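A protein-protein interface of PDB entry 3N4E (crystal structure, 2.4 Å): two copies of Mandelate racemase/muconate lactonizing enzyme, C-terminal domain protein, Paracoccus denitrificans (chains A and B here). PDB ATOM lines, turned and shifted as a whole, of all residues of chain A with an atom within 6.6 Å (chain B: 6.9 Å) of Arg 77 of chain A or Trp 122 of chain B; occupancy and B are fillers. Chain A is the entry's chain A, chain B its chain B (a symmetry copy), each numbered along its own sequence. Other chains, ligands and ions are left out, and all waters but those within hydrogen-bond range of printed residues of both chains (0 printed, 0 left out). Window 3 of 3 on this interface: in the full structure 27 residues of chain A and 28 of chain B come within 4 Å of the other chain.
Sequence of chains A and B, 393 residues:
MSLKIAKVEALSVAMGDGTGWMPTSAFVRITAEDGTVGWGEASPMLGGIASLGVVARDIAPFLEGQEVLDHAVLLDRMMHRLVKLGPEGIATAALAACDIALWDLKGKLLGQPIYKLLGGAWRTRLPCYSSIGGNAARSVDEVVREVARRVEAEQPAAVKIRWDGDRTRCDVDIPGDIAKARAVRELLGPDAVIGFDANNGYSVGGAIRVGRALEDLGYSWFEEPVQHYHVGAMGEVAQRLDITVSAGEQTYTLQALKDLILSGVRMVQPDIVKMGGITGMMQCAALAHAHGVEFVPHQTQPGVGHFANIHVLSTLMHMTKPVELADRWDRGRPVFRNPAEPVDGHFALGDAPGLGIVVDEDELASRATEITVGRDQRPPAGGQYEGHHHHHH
Among the printed residues, pairs that only touch across the chains: Val 73 of chain A with Gly 120 of chain B, Val 73 of chain A with Ala 121 of chain B, Val 73 of chain A with Trp 122 of chain B, Asp 76 of chain A with Trp 122 of chain B and Arg 77 of chain A with Trp 122 of chain B.
Hydrophobic or aromatic side chains of chain B within 4 Å of the printed part of chain A: Trp 122 and Met 317.
Of the 12 printed residues of chain A, 4 touch a printed residue of chain B.
Among the printed residues, 6 pairs touch across the chains.
Arg 77 of chain A touches one residue of chain B.
Printed residues of chain B within 4 Å of His 80 of chain A: Met 317.
Printed residues of chain A within 4 Å of Met 317 of chain B: His 80 (3.4 Å).
The nearest residue of chain B that does not touch Arg 77 of chain A is Met 317 of chain B (5.3 Å).
ND1 of His 80 of chain A sits at hydrogen-bond distance from O of Asp 76 of chain A, 2.8 Å away.
O of Tyr 115 of chain B sits at hydrogen-bond distance from N of Gly 120 of chain B (3.0 Å).
N of Trp 122 of chain B is in hydrogen-bond range of O of Ser 314 of chain B (2.8 Å).
The indole nitrogen (NE1) of Trp 122 of chain B sits close to the backbone carbonyl oxygen (O) of Thr 315 of chain B.
A ring nitrogen (ND1) of His 80 of chain A lies close to the side-chain sulfur of Met 317 of chain B (3.6 Å).
No position is printed for both chains.
Of the 6 pairs that touch across the chains among the printed residues, none has its exchanged pair printed and touching as well.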
ATOM      1  N   PHE A  62      -8.887  -1.425  18.059  1.00  0.00           N
ATOM      2  CA  PHE A  62      -8.592  -2.817  18.349  1.00  0.00           C
ATOM      3  C   PHE A  62      -7.608  -2.973  19.499  1.00  0.00           C
ATOM      4  O   PHE A  62      -7.735  -3.893  20.298  1.00  0.00           O
ATOM      5  CB  PHE A  62      -8.054  -3.524  17.101  1.00  0.00           C
ATOM      6  CG  PHE A  62      -7.460  -4.871  17.380  1.00  0.00           C
ATOM      7  CD1 PHE A  62      -8.278  -5.986  17.538  1.00  0.00           C
ATOM      8  CD2 PHE A  62      -6.078  -5.027  17.502  1.00  0.00           C
ATOM      9  CE1 PHE A  62      -7.725  -7.246  17.805  1.00  0.00           C
ATOM     10  CE2 PHE A  62      -5.520  -6.272  17.765  1.00  0.00           C
ATOM     11  CZ  PHE A  62      -6.344  -7.383  17.919  1.00  0.00           C
ATOM     12  N   ALA A  72       3.050  -9.110  19.893  1.00  0.00           N
ATOM     13  CA  ALA A  72       3.283  -9.911  18.702  1.00  0.00           C
ATOM     14  C   ALA A  72       1.998 -10.535  18.176  1.00  0.00           C
ATOM     15  O   ALA A  72       1.739 -10.503  16.971  1.00  0.00           O
ATOM     16  CB  ALA A  72       4.327 -10.973  18.974  1.00  0.00           C
ATOM     17  N   VAL A  73       1.194 -11.095  19.080  1.00  0.00           N
ATOM     18  CA  VAL A  73      -0.077 -11.706  18.711  1.00  0.00           C
ATOM     19  C   VAL A  73      -1.014 -10.623  18.172  1.00  0.00           C
ATOM     20  O   VAL A  73      -1.614 -10.780  17.112  1.00  0.00           O
ATOM     21  CB  VAL A  73      -0.714 -12.452  19.923  1.00  0.00           C
ATOM     22  CG1 VAL A  73      -2.187 -12.786  19.685  1.00  0.00           C
ATOM     23  CG2 VAL A  73       0.066 -13.717  20.221  1.00  0.00           C
ATOM     24  N   LEU A  74      -1.117  -9.523  18.909  1.00  0.00           N
ATOM     25  CA  LEU A  74      -1.986  -8.411  18.558  1.00  0.00           C
ATOM     26  C   LEU A  74      -1.699  -7.860  17.156  1.00  0.00           C
ATOM     27  O   LEU A  74      -2.615  -7.656  16.361  1.00  0.00           O
ATOM     28  CB  LEU A  74      -1.843  -7.291  19.600  1.00  0.00           C
ATOM     29  CG  LEU A  74      -2.337  -7.569  21.020  1.00  0.00           C
ATOM     30  CD1 LEU A  74      -1.978  -6.407  21.955  1.00  0.00           C
ATOM     31  CD2 LEU A  74      -3.830  -7.824  21.005  1.00  0.00           C
ATOM     32  N   LEU A  75      -0.425  -7.639  16.853  1.00  0.00           N
ATOM     33  CA  LEU A  75      -0.061  -7.000  15.593  1.00  0.00           C
ATOM     34  C   LEU A  75      -0.063  -7.967  14.405  1.00  0.00           C
ATOM     35  O   LEU A  75      -0.391  -7.555  13.291  1.00  0.00           O
ATOM     36  CB  LEU A  75       1.236  -6.176  15.735  1.00  0.00           C
ATOM     37  CG  LEU A  75       1.033  -4.986  16.708  1.00  0.00           C
ATOM     38  CD1 LEU A  75       2.284  -4.143  16.919  1.00  0.00           C
ATOM     39  CD2 LEU A  75      -0.121  -4.082  16.283  1.00  0.00           C
ATOM     40  N   ASP A  76       0.266  -9.240  14.646  1.00  0.00           N
ATOM     41  CA  ASP A  76       0.051 -10.303  13.644  1.00  0.00           C
ATOM     42  C   ASP A  76      -1.433 -10.460  13.303  1.00  0.00           C
ATOM     43  O   ASP A  76      -1.790 -10.645  12.144  1.00  0.00           O
ATOM     44  CB  ASP A  76       0.600 -11.659  14.114  1.00  0.00           C
ATOM     45  CG  ASP A  76       2.117 -11.744  14.042  1.00  0.00           C
ATOM     46  OD1 ASP A  76       2.778 -10.689  13.862  1.00  0.00           O
ATOM     47  OD2 ASP A  76       2.654 -12.871  14.177  1.00  0.00           O
ATOM     48  N   ARG A  77      -2.288 -10.395  14.318  1.00  0.00           N
ATOM     49  CA  ARG A  77      -3.722 -10.456  14.109  1.00  0.00           C
ATOM     50  C   ARG A  77      -4.166  -9.221  13.340  1.00  0.00           C
ATOM     51  O   ARG A  77      -4.954  -9.309  12.401  1.00  0.00           O
ATOM     52  CB  ARG A  77      -4.453 -10.604  15.448  1.00  0.00           C
ATOM     53  CG  ARG A  77      -5.940 -10.276  15.428  1.00  0.00           C
ATOM     54  CD  ARG A  77      -6.796 -11.370  16.086  1.00  0.00           C
ATOM     55  NE  ARG A  77      -6.266 -11.884  17.361  1.00  0.00           N
ATOM     56  CZ  ARG A  77      -6.387 -13.155  17.749  1.00  0.00           C
ATOM     57  NH1 ARG A  77      -5.895 -13.553  18.917  1.00  0.00           N
ATOM     58  NH2 ARG A  77      -6.996 -14.033  16.959  1.00  0.00           N
ATOM     59  N   MET A  78      -3.624  -8.075  13.723  1.00  0.00           N
ATOM     60  CA  MET A  78      -3.956  -6.821  13.079  1.00  0.00           C
ATOM     61  C   MET A  78      -3.520  -6.782  11.624  1.00  0.00           C
ATOM     62  O   MET A  78      -4.235  -6.260  10.773  1.00  0.00           O
ATOM     63  CB  MET A  78      -3.376  -5.645  13.859  1.00  0.00           C
ATOM     64  CG  MET A  78      -4.041  -4.341  13.529  1.00  0.00           C
ATOM     65  SD  MET A  78      -5.964  -4.200  13.939  1.00  0.00           S
ATOM     66  CE  MET A  78      -6.590  -6.047  14.173  1.00  0.00           C
ATOM     67  N   MET A  79      -2.361  -7.361  11.336  1.00  0.00           N
ATOM     68  CA  MET A  79      -1.867  -7.415   9.963  1.00  0.00           C
ATOM     69  C   MET A  79      -2.789  -8.247   9.070  1.00  0.00           C
ATOM     70  O   MET A  79      -3.056  -7.876   7.932  1.00  0.00           O
ATOM     71  CB  MET A  79      -0.425  -7.932   9.898  1.00  0.00           C
ATOM     72  CG  MET A  79       0.218  -7.817   8.514  1.00  0.00           C
ATOM     73  SD  MET A  79      -0.423  -9.220   7.263  1.00  0.00           S
ATOM     74  CE  MET A  79       0.889 -10.634   7.675  1.00  0.00           C
ATOM     75  N   HIS A  80      -3.290  -9.366   9.589  1.00  0.00           N
ATOM     76  CA  HIS A  80      -4.198 -10.217   8.817  1.00  0.00           C
ATOM     77  C   HIS A  80      -5.604  -9.660   8.635  1.00  0.00           C
ATOM     78  O   HIS A  80      -6.303 -10.055   7.710  1.00  0.00           O
ATOM     79  CB  HIS A  80      -4.218 -11.640   9.367  1.00  0.00           C
ATOM     80  CG  HIS A  80      -2.959 -12.386   9.075  1.00  0.00           C
ATOM     81  ND1 HIS A  80      -1.854 -12.322   9.892  1.00  0.00           N
ATOM     82  CD2 HIS A  80      -2.603 -13.148   8.016  1.00  0.00           C
ATOM     83  CE1 HIS A  80      -0.881 -13.037   9.362  1.00  0.00           C
ATOM     84  NE2 HIS A  80      -1.311 -13.551   8.225  1.00  0.00           N
ATOM     85  N   ARG A  81      -6.008  -8.742   9.507  1.00  0.00           N
ATOM     86  CA  ARG A  81      -7.233  -7.970   9.313  1.00  0.00           C
ATOM     87  C   ARG A  81      -7.072  -6.848   8.280  1.00  0.00           C
ATOM     88  O   ARG A  81      -8.020  -6.499   7.579  1.00  0.00           O
ATOM     89  CB  ARG A  81      -7.690  -7.369  10.633  1.00  0.00           C
ATOM     90  CG  ARG A  81      -8.502  -8.302  11.460  1.00  0.00           C
ATOM     91  CD  ARG A  81      -9.361  -7.504  12.391  1.00  0.00           C
ATOM     92  NE  ARG A  81      -9.615  -8.224  13.637  1.00  0.00           N
ATOM     93  CZ  ARG A  81     -10.235  -7.695  14.685  1.00  0.00           C
ATOM     94  NH1 ARG A  81     -10.670  -6.438  14.640  1.00  0.00           N
ATOM     95  NH2 ARG A  81     -10.417  -8.420  15.782  1.00  0.00           N
ATOM     96  N   LEU A  82      -5.860  -6.305   8.212  1.00  0.00           N
ATOM     97  CA  LEU A  82      -5.501  -5.183   7.356  1.00  0.00           C
ATOM     98  C   LEU A  82      -4.866  -5.636   6.054  1.00  0.00           C
ATOM     99  O   LEU A  82      -4.425  -4.803   5.259  1.00  0.00           O
ATOM    100  CB  LEU A  82      -4.490  -4.284   8.084  1.00  0.00           C
ATOM    101  CG  LEU A  82      -4.909  -3.149   9.021  1.00  0.00           C
ATOM    102  CD1 LEU A  82      -6.135  -3.470   9.878  1.00  0.00           C
ATOM    103  CD2 LEU A  82      -3.731  -2.748   9.900  1.00  0.00           C
ATOM    104  N   TYR B 115       5.954 -17.088  27.601  1.00  0.00           N
ATOM    105  CA  TYR B 115       5.193 -16.642  26.428  1.00  0.00           C
ATOM    106  C   TYR B 115       4.832 -15.146  26.511  1.00  0.00           C
ATOM    107  O   TYR B 115       4.633 -14.487  25.483  1.00  0.00           O
ATOM    108  CB  TYR B 115       3.959 -17.529  26.164  1.00  0.00           C
ATOM    109  CG  TYR B 115       2.870 -17.409  27.194  1.00  0.00           C
ATOM    110  CD1 TYR B 115       1.865 -16.445  27.070  1.00  0.00           C
ATOM    111  CD2 TYR B 115       2.848 -18.245  28.306  1.00  0.00           C
ATOM    112  CE1 TYR B 115       0.850 -16.324  28.035  1.00  0.00           C
ATOM    113  CE2 TYR B 115       1.855 -18.131  29.270  1.00  0.00           C
ATOM    114  CZ  TYR B 115       0.863 -17.174  29.123  1.00  0.00           C
ATOM    115  OH  TYR B 115      -0.114 -17.074  30.080  1.00  0.00           O
ATOM    116  N   GLY B 120       3.197 -12.828  23.495  1.00  0.00           N
ATOM    117  CA  GLY B 120       1.829 -13.297  23.672  1.00  0.00           C
ATOM    118  C   GLY B 120       1.548 -14.708  23.177  1.00  0.00           C
ATOM    119  O   GLY B 120       2.246 -15.226  22.307  1.00  0.00           O
ATOM    120  N   ALA B 121       0.516 -15.327  23.744  1.00  0.00           N
ATOM    121  CA  ALA B 121       0.062 -16.631  23.292  1.00  0.00           C
ATOM    122  C   ALA B 121      -1.178 -16.455  22.451  1.00  0.00           C
ATOM    123  O   ALA B 121      -2.084 -15.678  22.802  1.00  0.00           O
ATOM    124  CB  ALA B 121      -0.249 -17.540  24.476  1.00  0.00           C
ATOM    125  N   TRP B 122      -1.210 -17.186  21.339  1.00  0.00           N
ATOM    126  CA  TRP B 122      -2.427 -17.371  20.561  1.00  0.00           C
ATOM    127  C   TRP B 122      -3.396 -18.279  21.316  1.00  0.00           C
ATOM    128  O   TRP B 122      -4.622 -18.199  21.140  1.00  0.00           O
ATOM    129  CB  TRP B 122      -2.088 -17.984  19.202  1.00  0.00           C
ATOM    130  CG  TRP B 122      -1.324 -17.051  18.301  1.00  0.00           C
ATOM    131  CD1 TRP B 122       0.040 -16.962  18.173  1.00  0.00           C
ATOM    132  CD2 TRP B 122      -1.872 -16.067  17.411  1.00  0.00           C
ATOM    133  NE1 TRP B 122       0.365 -16.003  17.252  1.00  0.00           N
ATOM    134  CE2 TRP B 122      -0.785 -15.429  16.776  1.00  0.00           C
ATOM    135  CE3 TRP B 122      -3.174 -15.675  17.081  1.00  0.00           C
ATOM    136  CZ2 TRP B 122      -0.958 -14.418  15.830  1.00  0.00           C
ATOM    137  CZ3 TRP B 122      -3.350 -14.671  16.147  1.00  0.00           C
ATOM    138  CH2 TRP B 122      -2.247 -14.053  15.526  1.00  0.00           C
ATOM    139  N   ARG B 123      -2.845 -19.161  22.142  1.00  0.00           N
ATOM    140  CA  ARG B 123      -3.677 -20.090  22.920  1.00  0.00           C
ATOM    141  C   ARG B 123      -2.912 -20.590  24.143  1.00  0.00           C
ATOM    142  O   ARG B 123      -1.679 -20.614  24.142  1.00  0.00           O
ATOM    143  CB  ARG B 123      -4.129 -21.260  22.043  1.00  0.00           C
ATOM    144  CG  ARG B 123      -2.981 -22.169  21.652  1.00  0.00           C
ATOM    145  CD  ARG B 123      -3.049 -22.588  20.216  1.00  0.00           C
ATOM    146  NE  ARG B 123      -1.739 -22.329  19.682  1.00  0.00           N
ATOM    147  CZ  ARG B 123      -1.456 -21.707  18.546  1.00  0.00           C
ATOM    148  NH1 ARG B 123      -0.184 -21.528  18.257  1.00  0.00           N
ATOM    149  NH2 ARG B 123      -2.393 -21.315  17.704  1.00  0.00           N
ATOM    150  N   THR B 124      -3.641 -20.976  25.182  1.00  0.00           N
ATOM    151  CA  THR B 124      -3.028 -21.501  26.407  1.00  0.00           C
ATOM    152  C   THR B 124      -3.521 -22.932  26.661  1.00  0.00           C
ATOM    153  O   THR B 124      -3.270 -23.536  27.703  1.00  0.00           O
ATOM    154  CB  THR B 124      -3.346 -20.601  27.611  1.00  0.00           C
ATOM    155  OG1 THR B 124      -4.769 -20.407  27.699  1.00  0.00           O
ATOM    156  CG2 THR B 124      -2.657 -19.237  27.466  1.00  0.00           C
ATOM    157  N   ARG B 125      -4.246 -23.453  25.684  1.00  0.00           N
ATOM    158  CA  ARG B 125      -4.692 -24.834  25.680  1.00  0.00           C
ATOM    159  C   ARG B 125      -4.276 -25.396  24.342  1.00  0.00           C
ATOM    160  O   ARG B 125      -4.738 -24.938  23.283  1.00  0.00           O
ATOM    161  CB  ARG B 125      -6.205 -24.930  25.830  1.00  0.00           C
ATOM    162  CG  ARG B 125      -6.696 -24.725  27.224  1.00  0.00           C
ATOM    163  CD  ARG B 125      -7.936 -25.557  27.429  1.00  0.00           C
ATOM    164  NE  ARG B 125      -7.616 -26.832  28.070  1.00  0.00           N
ATOM    165  CZ  ARG B 125      -8.438 -27.879  28.140  1.00  0.00           C
ATOM    166  NH1 ARG B 125      -9.647 -27.833  27.589  1.00  0.00           N
ATOM    167  NH2 ARG B 125      -8.045 -28.981  28.770  1.00  0.00           N
ATOM    168  N   LEU B 313       5.361 -22.830  21.207  1.00  0.00           N
ATOM    169  CA  LEU B 313       4.204 -23.157  20.385  1.00  0.00           C
ATOM    170  C   LEU B 313       2.974 -22.294  20.653  1.00  0.00           C
ATOM    171  O   LEU B 313       2.192 -22.044  19.739  1.00  0.00           O
ATOM    172  CB  LEU B 313       3.881 -24.653  20.456  1.00  0.00           C
ATOM    173  CG  LEU B 313       4.934 -25.488  19.694  1.00  0.00           C
ATOM    174  CD1 LEU B 313       4.842 -26.972  20.019  1.00  0.00           C
ATOM    175  CD2 LEU B 313       4.840 -25.267  18.181  1.00  0.00           C
ATOM    176  N   SER B 314       2.802 -21.812  21.879  1.00  0.00           N
ATOM    177  CA  SER B 314       1.699 -20.885  22.128  1.00  0.00           C
ATOM    178  C   SER B 314       1.844 -19.613  21.283  1.00  0.00           C
ATOM    179  O   SER B 314       0.836 -19.001  20.916  1.00  0.00           O
ATOM    180  CB  SER B 314       1.571 -20.547  23.611  1.00  0.00           C
ATOM    181  OG  SER B 314       2.668 -19.769  24.037  1.00  0.00           O
ATOM    182  N   THR B 315       3.084 -19.237  20.961  1.00  0.00           N
ATOM    183  CA  THR B 315       3.372 -18.067  20.114  1.00  0.00           C
ATOM    184  C   THR B 315       3.167 -18.318  18.616  1.00  0.00           C
ATOM    185  O   THR B 315       3.154 -17.375  17.831  1.00  0.00           O
ATOM    186  CB  THR B 315       4.834 -17.496  20.319  1.00  0.00           C
ATOM    187  OG1 THR B 315       5.790 -18.328  19.666  1.00  0.00           O
ATOM    188  CG2 THR B 315       5.206 -17.388  21.794  1.00  0.00           C
ATOM    189  N   LEU B 316       3.016 -19.577  18.213  1.00  0.00           N
ATOM    190  CA  LEU B 316       2.949 -19.906  16.787  1.00  0.00           C
ATOM    191  C   LEU B 316       1.578 -19.614  16.184  1.00  0.00           C
ATOM    192  O   LEU B 316       0.607 -20.285  16.492  1.00  0.00           O
ATOM    193  CB  LEU B 316       3.350 -21.369  16.534  1.00  0.00           C
ATOM    194  CG  LEU B 316       3.355 -21.828  15.065  1.00  0.00           C
ATOM    195  CD1 LEU B 316       4.484 -21.167  14.285  1.00  0.00           C
ATOM    196  CD2 LEU B 316       3.455 -23.332  14.962  1.00  0.00           C
ATOM    197  N   MET B 317       1.501 -18.613  15.313  1.00  0.00           N
ATOM    198  CA  MET B 317       0.223 -18.261  14.690  1.00  0.00           C
ATOM    199  C   MET B 317      -0.363 -19.411  13.874  1.00  0.00           C
ATOM    200  O   MET B 317      -1.433 -19.915  14.179  1.00  0.00           O
ATOM    201  CB  MET B 317       0.355 -17.011  13.826  1.00  0.00           C
ATOM    202  CG  MET B 317      -0.938 -16.644  13.113  1.00  0.00           C
ATOM    203  SD  MET B 317      -0.769 -14.999  12.076  1.00  0.00           S
ATOM    204  CE  MET B 317       0.750 -15.516  10.935  1.00  0.00           C
ATOM    205  N   HIS B 318       0.343 -19.833  12.837  1.00  0.00           N
ATOM    206  CA  HIS B 318      -0.173 -20.883  11.976  1.00  0.00           C
ATOM    207  C   HIS B 318       0.244 -22.261  12.479  1.00  0.00           C
ATOM    208  O   HIS B 318       1.015 -22.967  11.836  1.00  0.00           O
ATOM    209  CB  HIS B 318       0.243 -20.648  10.521  1.00  0.00           C
ATOM    210  CG  HIS B 318      -0.422 -19.461   9.899  1.00  0.00           C
ATOM    211  ND1 HIS B 318       0.152 -18.729   8.880  1.00  0.00           N
ATOM    212  CD2 HIS B 318      -1.610 -18.865  10.168  1.00  0.00           C
ATOM    213  CE1 HIS B 318      -0.661 -17.742   8.541  1.00  0.00           C
ATOM    214  NE2 HIS B 318      -1.739 -17.805   9.303  1.00  0.00           N
